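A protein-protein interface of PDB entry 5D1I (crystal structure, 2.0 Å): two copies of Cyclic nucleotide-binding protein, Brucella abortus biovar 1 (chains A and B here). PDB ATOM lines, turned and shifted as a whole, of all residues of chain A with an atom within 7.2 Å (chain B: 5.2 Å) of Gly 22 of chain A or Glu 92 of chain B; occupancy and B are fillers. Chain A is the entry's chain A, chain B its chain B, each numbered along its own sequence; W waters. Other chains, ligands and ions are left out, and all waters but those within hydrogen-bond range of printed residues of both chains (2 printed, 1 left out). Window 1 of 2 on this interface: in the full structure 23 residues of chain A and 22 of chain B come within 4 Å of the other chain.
The backbone carbonyl oxygen (O) of Thr 20 of chain A is in hydrogen-bond range of the backbone NH (N) of Ile 89 of chain B (3.2 Å).
The backbone NH of Gly 91 of chain B lies within hydrogen-bond range of the side-chain carboxylate of Glu 25 of chain A (2.9 Å).
OE1 of Glu 92 of chain A lies close to OE2 of Glu 92 of chain B (2.8 Å).
N of Leu 23 of chain A sits at hydrogen-bond distance from OE2 of Glu 92 of chain A (3.0 Å).
The backbone NH of Gly 22 of chain B sits at hydrogen-bond distance from the side-chain carboxylate of Glu 92 of chain B, 3.4 Å away.
N of Leu 23 of chain B lies within hydrogen-bond range of OE2 of Glu 92 of chain B, at 2.9 Å.
Gly 22 of chain A touches Ile 89 of chain B (CA to O, 3.8 Å).
Glu 92 of chain B touches Gly 22 of chain A (OE1 to CA, 3.4 Å).
Glu 92 of chain B touches Leu 23 of chain A (OE1 to N, 3.6 Å).
Glu 25 of chain A touches Ile 89 of chain B (CB to O, 3.9 Å).
Leu 90 of chain B touches Glu 25 of chain A (CB to OE2, 3.4 Å).
Gly 22 of chain B touches Ile 89 of chain A (CA to CG2, 3.8 Å).
Glu 92 of chain A touches Gly 22 of chain B.
Leu 23 of chain B touches Met 93 of chain A.
CE of Met 93 of chain A touches SD of Met 93 of chain B, 3.996 Å away.
Gly 19 of chain A touches none of the printed residues of chain B.
Val 21 of chain A touches none of the printed residues of chain B.
Gly 22 of chain A touches two residues of chain B.
Printed residues of chain B within 4 Å of Leu 23 of chain A: Glu 92.
Of the printed residues of chain A, Gly 22 of chain B touches Ile 89 (3.8 Å) and Glu 92 (3.2 Å).
Of the printed residues of chain A, Leu 90 of chain B touches Glu 25.
Printed residues of chain A within 4 Å of Gly 91 of chain B: Glu 25.
Glu 92 of chain B touches just these residues of chain A: Gly 22 (3.4 Å), Leu 23 (3.6 Å) and Glu 92 (2.8 Å).
The nearest printed residue of chain B that does not touch Gly 22 of chain A is Gly 91 of chain B (5.6 Å).
Printed residues of chain B that touch a printed residue of chain A: Gly 22, Leu 23, Ile 89, Leu 90, Gly 91, Glu 92 and Met 93.
Gly 22 of chain A touches Ile 89 of chain B, and with the chains exchanged Ile 89 of chain A touches Gly 22 of chain B.
Gly 22 of chain A touches Glu 92 of chain B, and with the chains exchanged Glu 92 of chain A touches Gly 22 of chain B.
Glu 92 of chain B touches its own counterpart, Glu 92 of chain A.
Met 93 of chain A touches Leu 23 of chain B, but with the chains exchanged Leu 23 of chain A does not touch Met 93 of chain B (4.7 Å).
6 positions are printed for both chains.
Water W1 lies within hydrogen-bond range of O of Ile 89 of chain A (2.8 Å), N of Glu 92 of chain A (3.0 Å) and O of Gly 22 of chain B (3.3 Å).
Water W2 lies within hydrogen-bond range of N of Gly 22 of chain A (3.0 Å), OE2 of Glu 92 of chain A (3.1 Å) and N of Gly 22 of chain B (3.1 Å).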
ATOM      1  N   LEU A  18     -21.823  -7.182 -15.662  1.00  0.00           N
ATOM      2  CA  LEU A  18     -23.117  -7.722 -15.254  1.00  0.00           C
ATOM      3  C   LEU A  18     -23.123  -8.094 -13.777  1.00  0.00           C
ATOM      4  O   LEU A  18     -24.160  -8.039 -13.121  1.00  0.00           O
ATOM      5  CB  LEU A  18     -23.482  -8.941 -16.101  1.00  0.00           C
ATOM      6  CG  LEU A  18     -23.805  -8.674 -17.573  1.00  0.00           C
ATOM      7  CD1 LEU A  18     -23.937  -9.982 -18.323  1.00  0.00           C
ATOM      8  CD2 LEU A  18     -25.077  -7.854 -17.712  1.00  0.00           C
ATOM      9  N   GLY A  19     -21.956  -8.466 -13.260  1.00  0.00           N
ATOM     10  CA  GLY A  19     -21.825  -8.873 -11.872  1.00  0.00           C
ATOM     11  C   GLY A  19     -21.941  -7.739 -10.867  1.00  0.00           C
ATOM     12  O   GLY A  19     -22.046  -7.983  -9.669  1.00  0.00           O
ATOM     13  N   THR A  20     -21.918  -6.499 -11.345  1.00  0.00           N
ATOM     14  CA  THR A  20     -22.075  -5.345 -10.462  1.00  0.00           C
ATOM     15  C   THR A  20     -23.541  -4.941 -10.323  1.00  0.00           C
ATOM     16  O   THR A  20     -23.905  -4.168  -9.433  1.00  0.00           O
ATOM     17  CB  THR A  20     -21.280  -4.132 -10.969  1.00  0.00           C
ATOM     18  OG1 THR A  20     -21.771  -3.741 -12.260  1.00  0.00           O
ATOM     19  CG2 THR A  20     -19.797  -4.462 -11.066  1.00  0.00           C
ATOM     20  N   VAL A  21     -24.379  -5.458 -11.211  1.00  0.00           N
ATOM     21  CA  VAL A  21     -25.796  -5.110 -11.223  1.00  0.00           C
ATOM     22  C   VAL A  21     -26.513  -5.714 -10.020  1.00  0.00           C
ATOM     23  O   VAL A  21     -26.365  -6.896  -9.738  1.00  0.00           O
ATOM     24  CB  VAL A  21     -26.460  -5.584 -12.527  1.00  0.00           C
ATOM     25  CG1 VAL A  21     -27.947  -5.312 -12.509  1.00  0.00           C
ATOM     26  CG2 VAL A  21     -25.810  -4.902 -13.715  1.00  0.00           C
ATOM     27  N   GLY A  22     -27.276  -4.890  -9.304  1.00  0.00           N
ATOM     28  CA  GLY A  22     -27.957  -5.321  -8.094  1.00  0.00           C
ATOM     29  C   GLY A  22     -28.796  -6.576  -8.246  1.00  0.00           C
ATOM     30  O   GLY A  22     -28.763  -7.468  -7.395  1.00  0.00           O
ATOM     31  N   LEU A  23     -29.542  -6.656  -9.339  1.00  0.00           N
ATOM     32  CA  LEU A  23     -30.420  -7.798  -9.568  1.00  0.00           C
ATOM     33  C   LEU A  23     -29.635  -9.086  -9.827  1.00  0.00           C
ATOM     34  O   LEU A  23     -30.137 -10.179  -9.579  1.00  0.00           O
ATOM     35  CB  LEU A  23     -31.362  -7.506 -10.737  1.00  0.00           C
ATOM     36  CG  LEU A  23     -32.605  -8.382 -10.884  1.00  0.00           C
ATOM     37  CD1 LEU A  23     -33.405  -8.387  -9.592  1.00  0.00           C
ATOM     38  CD2 LEU A  23     -33.459  -7.884 -12.044  1.00  0.00           C
ATOM     39  N   PHE A  24     -28.404  -8.956 -10.318  1.00  0.00           N
ATOM     40  CA  PHE A  24     -27.594 -10.123 -10.671  1.00  0.00           C
ATOM     41  C   PHE A  24     -26.553 -10.419  -9.599  1.00  0.00           C
ATOM     42  O   PHE A  24     -25.694 -11.283  -9.788  1.00  0.00           O
ATOM     43  CB  PHE A  24     -26.893  -9.915 -12.023  1.00  0.00           C
ATOM     44  CG  PHE A  24     -27.807  -9.433 -13.115  1.00  0.00           C
ATOM     45  CD1 PHE A  24     -29.128  -9.843 -13.165  1.00  0.00           C
ATOM     46  CD2 PHE A  24     -27.345  -8.561 -14.086  1.00  0.00           C
ATOM     47  CE1 PHE A  24     -29.973  -9.394 -14.162  1.00  0.00           C
ATOM     48  CE2 PHE A  24     -28.185  -8.111 -15.087  1.00  0.00           C
ATOM     49  CZ  PHE A  24     -29.499  -8.529 -15.125  1.00  0.00           C
ATOM     50  N   GLU A  25     -26.651  -9.704  -8.477  1.00  0.00           N
ATOM     51  CA  GLU A  25     -25.690  -9.789  -7.372  1.00  0.00           C
ATOM     52  C   GLU A  25     -25.326 -11.205  -6.934  1.00  0.00           C
ATOM     53  O   GLU A  25     -24.151 -11.527  -6.772  1.00  0.00           O
ATOM     54  CB  GLU A  25     -26.226  -9.034  -6.148  1.00  0.00           C
ATOM     55  CG  GLU A  25     -25.402  -9.267  -4.878  1.00  0.00           C
ATOM     56  CD  GLU A  25     -26.176  -8.997  -3.591  1.00  0.00           C
ATOM     57  OE1 GLU A  25     -27.390  -8.690  -3.656  1.00  0.00           O
ATOM     58  OE2 GLU A  25     -25.563  -9.104  -2.507  1.00  0.00           O
ATOM     59  N   SER A  26     -26.333 -12.044  -6.728  1.00  0.00           N
ATOM     60  CA  SER A  26     -26.102 -13.362  -6.147  1.00  0.00           C
ATOM     61  C   SER A  26     -25.839 -14.449  -7.189  1.00  0.00           C
ATOM     62  O   SER A  26     -25.736 -15.626  -6.846  1.00  0.00           O
ATOM     63  CB  SER A  26     -27.295 -13.767  -5.282  1.00  0.00           C
ATOM     64  OG  SER A  26     -28.482 -13.803  -6.052  1.00  0.00           O
ATOM     65  N   ILE A  89     -27.411   0.805 -15.494  1.00  0.00           N
ATOM     66  CA  ILE A  89     -28.453  -0.045 -16.036  1.00  0.00           C
ATOM     67  C   ILE A  89     -29.749   0.744 -16.168  1.00  0.00           C
ATOM     68  O   ILE A  89     -30.121   1.517 -15.279  1.00  0.00           O
ATOM     69  CB  ILE A  89     -28.682  -1.313 -15.173  1.00  0.00           C
ATOM     70  CG1 ILE A  89     -29.747  -2.203 -15.810  1.00  0.00           C
ATOM     71  CG2 ILE A  89     -29.076  -0.955 -13.743  1.00  0.00           C
ATOM     72  CD1 ILE A  89     -29.824  -3.579 -15.198  1.00  0.00           C
ATOM     73  N   GLU A  92     -33.959  -1.870 -15.107  1.00  0.00           N
ATOM     74  CA  GLU A  92     -33.730  -3.060 -14.289  1.00  0.00           C
ATOM     75  C   GLU A  92     -35.036  -3.623 -13.733  1.00  0.00           C
ATOM     76  O   GLU A  92     -35.218  -4.838 -13.667  1.00  0.00           O
ATOM     77  CB  GLU A  92     -32.778  -2.753 -13.131  1.00  0.00           C
ATOM     78  CG  GLU A  92     -32.331  -3.996 -12.363  1.00  0.00           C
ATOM     79  CD  GLU A  92     -31.528  -3.650 -11.127  1.00  0.00           C
ATOM     80  OE1 GLU A  92     -31.960  -2.756 -10.377  1.00  0.00           O
ATOM     81  OE2 GLU A  92     -30.469  -4.266 -10.903  1.00  0.00           O
ATOM     82  N   MET A  93     -35.945  -2.731 -13.346  1.00  0.00           N
ATOM     83  CA  MET A  93     -37.217  -3.143 -12.761  1.00  0.00           C
ATOM     84  C   MET A  93     -38.117  -3.855 -13.771  1.00  0.00           C
ATOM     85  O   MET A  93     -39.017  -4.608 -13.392  1.00  0.00           O
ATOM     86  CB  MET A  93     -37.951  -1.935 -12.176  1.00  0.00           C
ATOM     87  CG  MET A  93     -37.301  -1.350 -10.933  1.00  0.00           C
ATOM     88  SD  MET A  93     -37.027  -2.683  -9.535  1.00  0.00           S
ATOM     89  CE  MET A  93     -35.093  -2.877  -9.672  1.00  0.00           C
ATOM     90  N   VAL B  21     -27.121   2.505 -10.222  1.00  0.00           N
ATOM     91  CA  VAL B  21     -28.025   1.582  -9.534  1.00  0.00           C
ATOM     92  C   VAL B  21     -29.431   1.603 -10.121  1.00  0.00           C
ATOM     93  O   VAL B  21     -29.997   2.668 -10.355  1.00  0.00           O
ATOM     94  CB  VAL B  21     -28.106   1.912  -8.030  1.00  0.00           C
ATOM     95  CG1 VAL B  21     -29.079   0.974  -7.312  1.00  0.00           C
ATOM     96  CG2 VAL B  21     -26.725   1.851  -7.406  1.00  0.00           C
ATOM     97  N   GLY B  22     -29.994   0.418 -10.339  1.00  0.00           N
ATOM     98  CA  GLY B  22     -31.303   0.285 -10.952  1.00  0.00           C
ATOM     99  C   GLY B  22     -32.411   1.107 -10.320  1.00  0.00           C
ATOM    100  O   GLY B  22     -33.148   1.805 -11.021  1.00  0.00           O
ATOM    101  N   LEU B  23     -32.533   1.034  -8.999  1.00  0.00           N
ATOM    102  CA  LEU B  23     -33.590   1.754  -8.287  1.00  0.00           C
ATOM    103  C   LEU B  23     -33.420   3.271  -8.351  1.00  0.00           C
ATOM    104  O   LEU B  23     -34.384   4.013  -8.159  1.00  0.00           O
ATOM    105  CB  LEU B  23     -33.642   1.312  -6.822  1.00  0.00           C
ATOM    106  CG  LEU B  23     -34.303  -0.034  -6.522  1.00  0.00           C
ATOM    107  CD1 LEU B  23     -34.224  -0.344  -5.029  1.00  0.00           C
ATOM    108  CD2 LEU B  23     -35.756  -0.058  -7.006  1.00  0.00           C
ATOM    109  N   ALA B  60     -28.743  -1.724   1.581  1.00  0.00           N
ATOM    110  CA  ALA B  60     -27.908  -2.111   0.461  1.00  0.00           C
ATOM    111  C   ALA B  60     -26.496  -1.559   0.654  1.00  0.00           C
ATOM    112  O   ALA B  60     -26.299  -0.564   1.355  1.00  0.00           O
ATOM    113  CB  ALA B  60     -28.511  -1.615  -0.850  1.00  0.00           C
ATOM    114  N   ILE B  89     -23.291  -3.435  -6.382  1.00  0.00           N
ATOM    115  CA  ILE B  89     -24.350  -3.159  -5.421  1.00  0.00           C
ATOM    116  C   ILE B  89     -24.840  -4.444  -4.742  1.00  0.00           C
ATOM    117  O   ILE B  89     -25.313  -5.367  -5.409  1.00  0.00           O
ATOM    118  CB  ILE B  89     -25.533  -2.457  -6.105  1.00  0.00           C
ATOM    119  CG1 ILE B  89     -25.023  -1.274  -6.932  1.00  0.00           C
ATOM    120  CG2 ILE B  89     -26.549  -2.000  -5.069  1.00  0.00           C
ATOM    121  CD1 ILE B  89     -25.305  -1.378  -8.422  1.00  0.00           C
ATOM    122  N   LEU B  90     -24.711  -4.512  -3.420  1.00  0.00           N
ATOM    123  CA  LEU B  90     -25.162  -5.686  -2.676  1.00  0.00           C
ATOM    124  C   LEU B  90     -26.475  -5.411  -1.937  1.00  0.00           C
ATOM    125  O   LEU B  90     -26.598  -4.412  -1.237  1.00  0.00           O
ATOM    126  CB  LEU B  90     -24.092  -6.143  -1.682  1.00  0.00           C
ATOM    127  CG  LEU B  90     -22.673  -6.366  -2.215  1.00  0.00           C
ATOM    128  CD1 LEU B  90     -21.770  -6.968  -1.140  1.00  0.00           C
ATOM    129  CD2 LEU B  90     -22.694  -7.249  -3.443  1.00  0.00           C
ATOM    130  N   GLY B  91     -27.452  -6.298  -2.099  1.00  0.00           N
ATOM    131  CA  GLY B  91     -28.718  -6.178  -1.395  1.00  0.00           C
ATOM    132  C   GLY B  91     -29.616  -5.048  -1.870  1.00  0.00           C
ATOM    133  O   GLY B  91     -30.289  -4.408  -1.067  1.00  0.00           O
ATOM    134  N   GLU B  92     -29.647  -4.808  -3.177  1.00  0.00           N
ATOM    135  CA  GLU B  92     -30.434  -3.705  -3.717  1.00  0.00           C
ATOM    136  C   GLU B  92     -31.923  -3.794  -3.381  1.00  0.00           C
ATOM    137  O   GLU B  92     -32.545  -2.787  -3.052  1.00  0.00           O
ATOM    138  CB  GLU B  92     -30.278  -3.618  -5.236  1.00  0.00           C
ATOM    139  CG  GLU B  92     -31.061  -2.461  -5.847  1.00  0.00           C
ATOM    140  CD  GLU B  92     -31.135  -2.522  -7.358  1.00  0.00           C
ATOM    141  OE1 GLU B  92     -30.897  -3.609  -7.919  1.00  0.00           O
ATOM    142  OE2 GLU B  92     -31.440  -1.484  -7.981  1.00  0.00           O
ATOM    143  N   MET B  93     -32.501  -4.986  -3.471  1.00  0.00           N
ATOM    144  CA  MET B  93     -33.949  -5.103  -3.291  1.00  0.00           C
ATOM    145  C   MET B  93     -34.349  -4.919  -1.825  1.00  0.00           C
ATOM    146  O   MET B  93     -35.532  -4.791  -1.515  1.00  0.00           O
ATOM    147  CB  MET B  93     -34.462  -6.445  -3.818  1.00  0.00           C
ATOM    148  CG  MET B  93     -34.424  -6.581  -5.347  1.00  0.00           C
ATOM    149  SD  MET B  93     -35.106  -5.017  -6.297  1.00  0.00           S
ATOM    150  CE  MET B  93     -36.889  -4.967  -5.545  1.00  0.00           C
ATOM    151  N   ALA B  94     -33.366  -4.884  -0.929  1.00  0.00           N
ATOM    152  CA  ALA B  94     -33.646  -4.604   0.480  1.00  0.00           C
ATOM    153  C   ALA B  94     -34.120  -3.162   0.661  1.00  0.00           C
ATOM    154  O   ALA B  94     -34.628  -2.795   1.722  1.00  0.00           O
ATOM    155  CB  ALA B  94     -32.415  -4.875   1.343  1.00  0.00           C
ATOM    156  N   LEU B  95     -33.950  -2.349  -0.381  1.00  0.00           N
ATOM    157  CA  LEU B  95     -34.437  -0.975  -0.368  1.00  0.00           C
ATOM    158  C   LEU B  95     -35.928  -0.915  -0.675  1.00  0.00           C
ATOM    159  O   LEU B  95     -36.572   0.116  -0.481  1.00  0.00           O
ATOM    160  CB  LEU B  95     -33.670  -0.122  -1.381  1.00  0.00           C
ATOM    161  CG  LEU B  95     -32.157  -0.007  -1.195  1.00  0.00           C
ATOM    162  CD1 LEU B  95     -31.563   0.916  -2.248  1.00  0.00           C
ATOM    163  CD2 LEU B  95     -31.823   0.485   0.210  1.00  0.00           C
ATOM    164  N   ILE B  96     -36.474  -2.024  -1.161  1.00  0.00           N
ATOM    165  CA  ILE B  96     -37.886  -2.082  -1.536  1.00  0.00           C
ATOM    166  C   ILE B  96     -38.721  -2.812  -0.487  1.00  0.00           C
ATOM    167  O   ILE B  96     -39.852  -2.423  -0.185  1.00  0.00           O
ATOM    168  CB  ILE B  96     -38.053  -2.765  -2.907  1.00  0.00           C
ATOM    169  CG1 ILE B  96     -37.503  -1.862  -4.009  1.00  0.00           C
ATOM    170  CG2 ILE B  96     -39.497  -3.056  -3.192  1.00  0.00           C
ATOM    171  CD1 ILE B  96     -38.159  -0.508  -4.060  1.00  0.00           C
HETATM  172  O   HOH W   1     -32.490   0.563 -14.019  1.00  0.00           O
HETATM  173  O   HOH W   2     -28.380  -2.220 -10.031  1.00  0.00           O
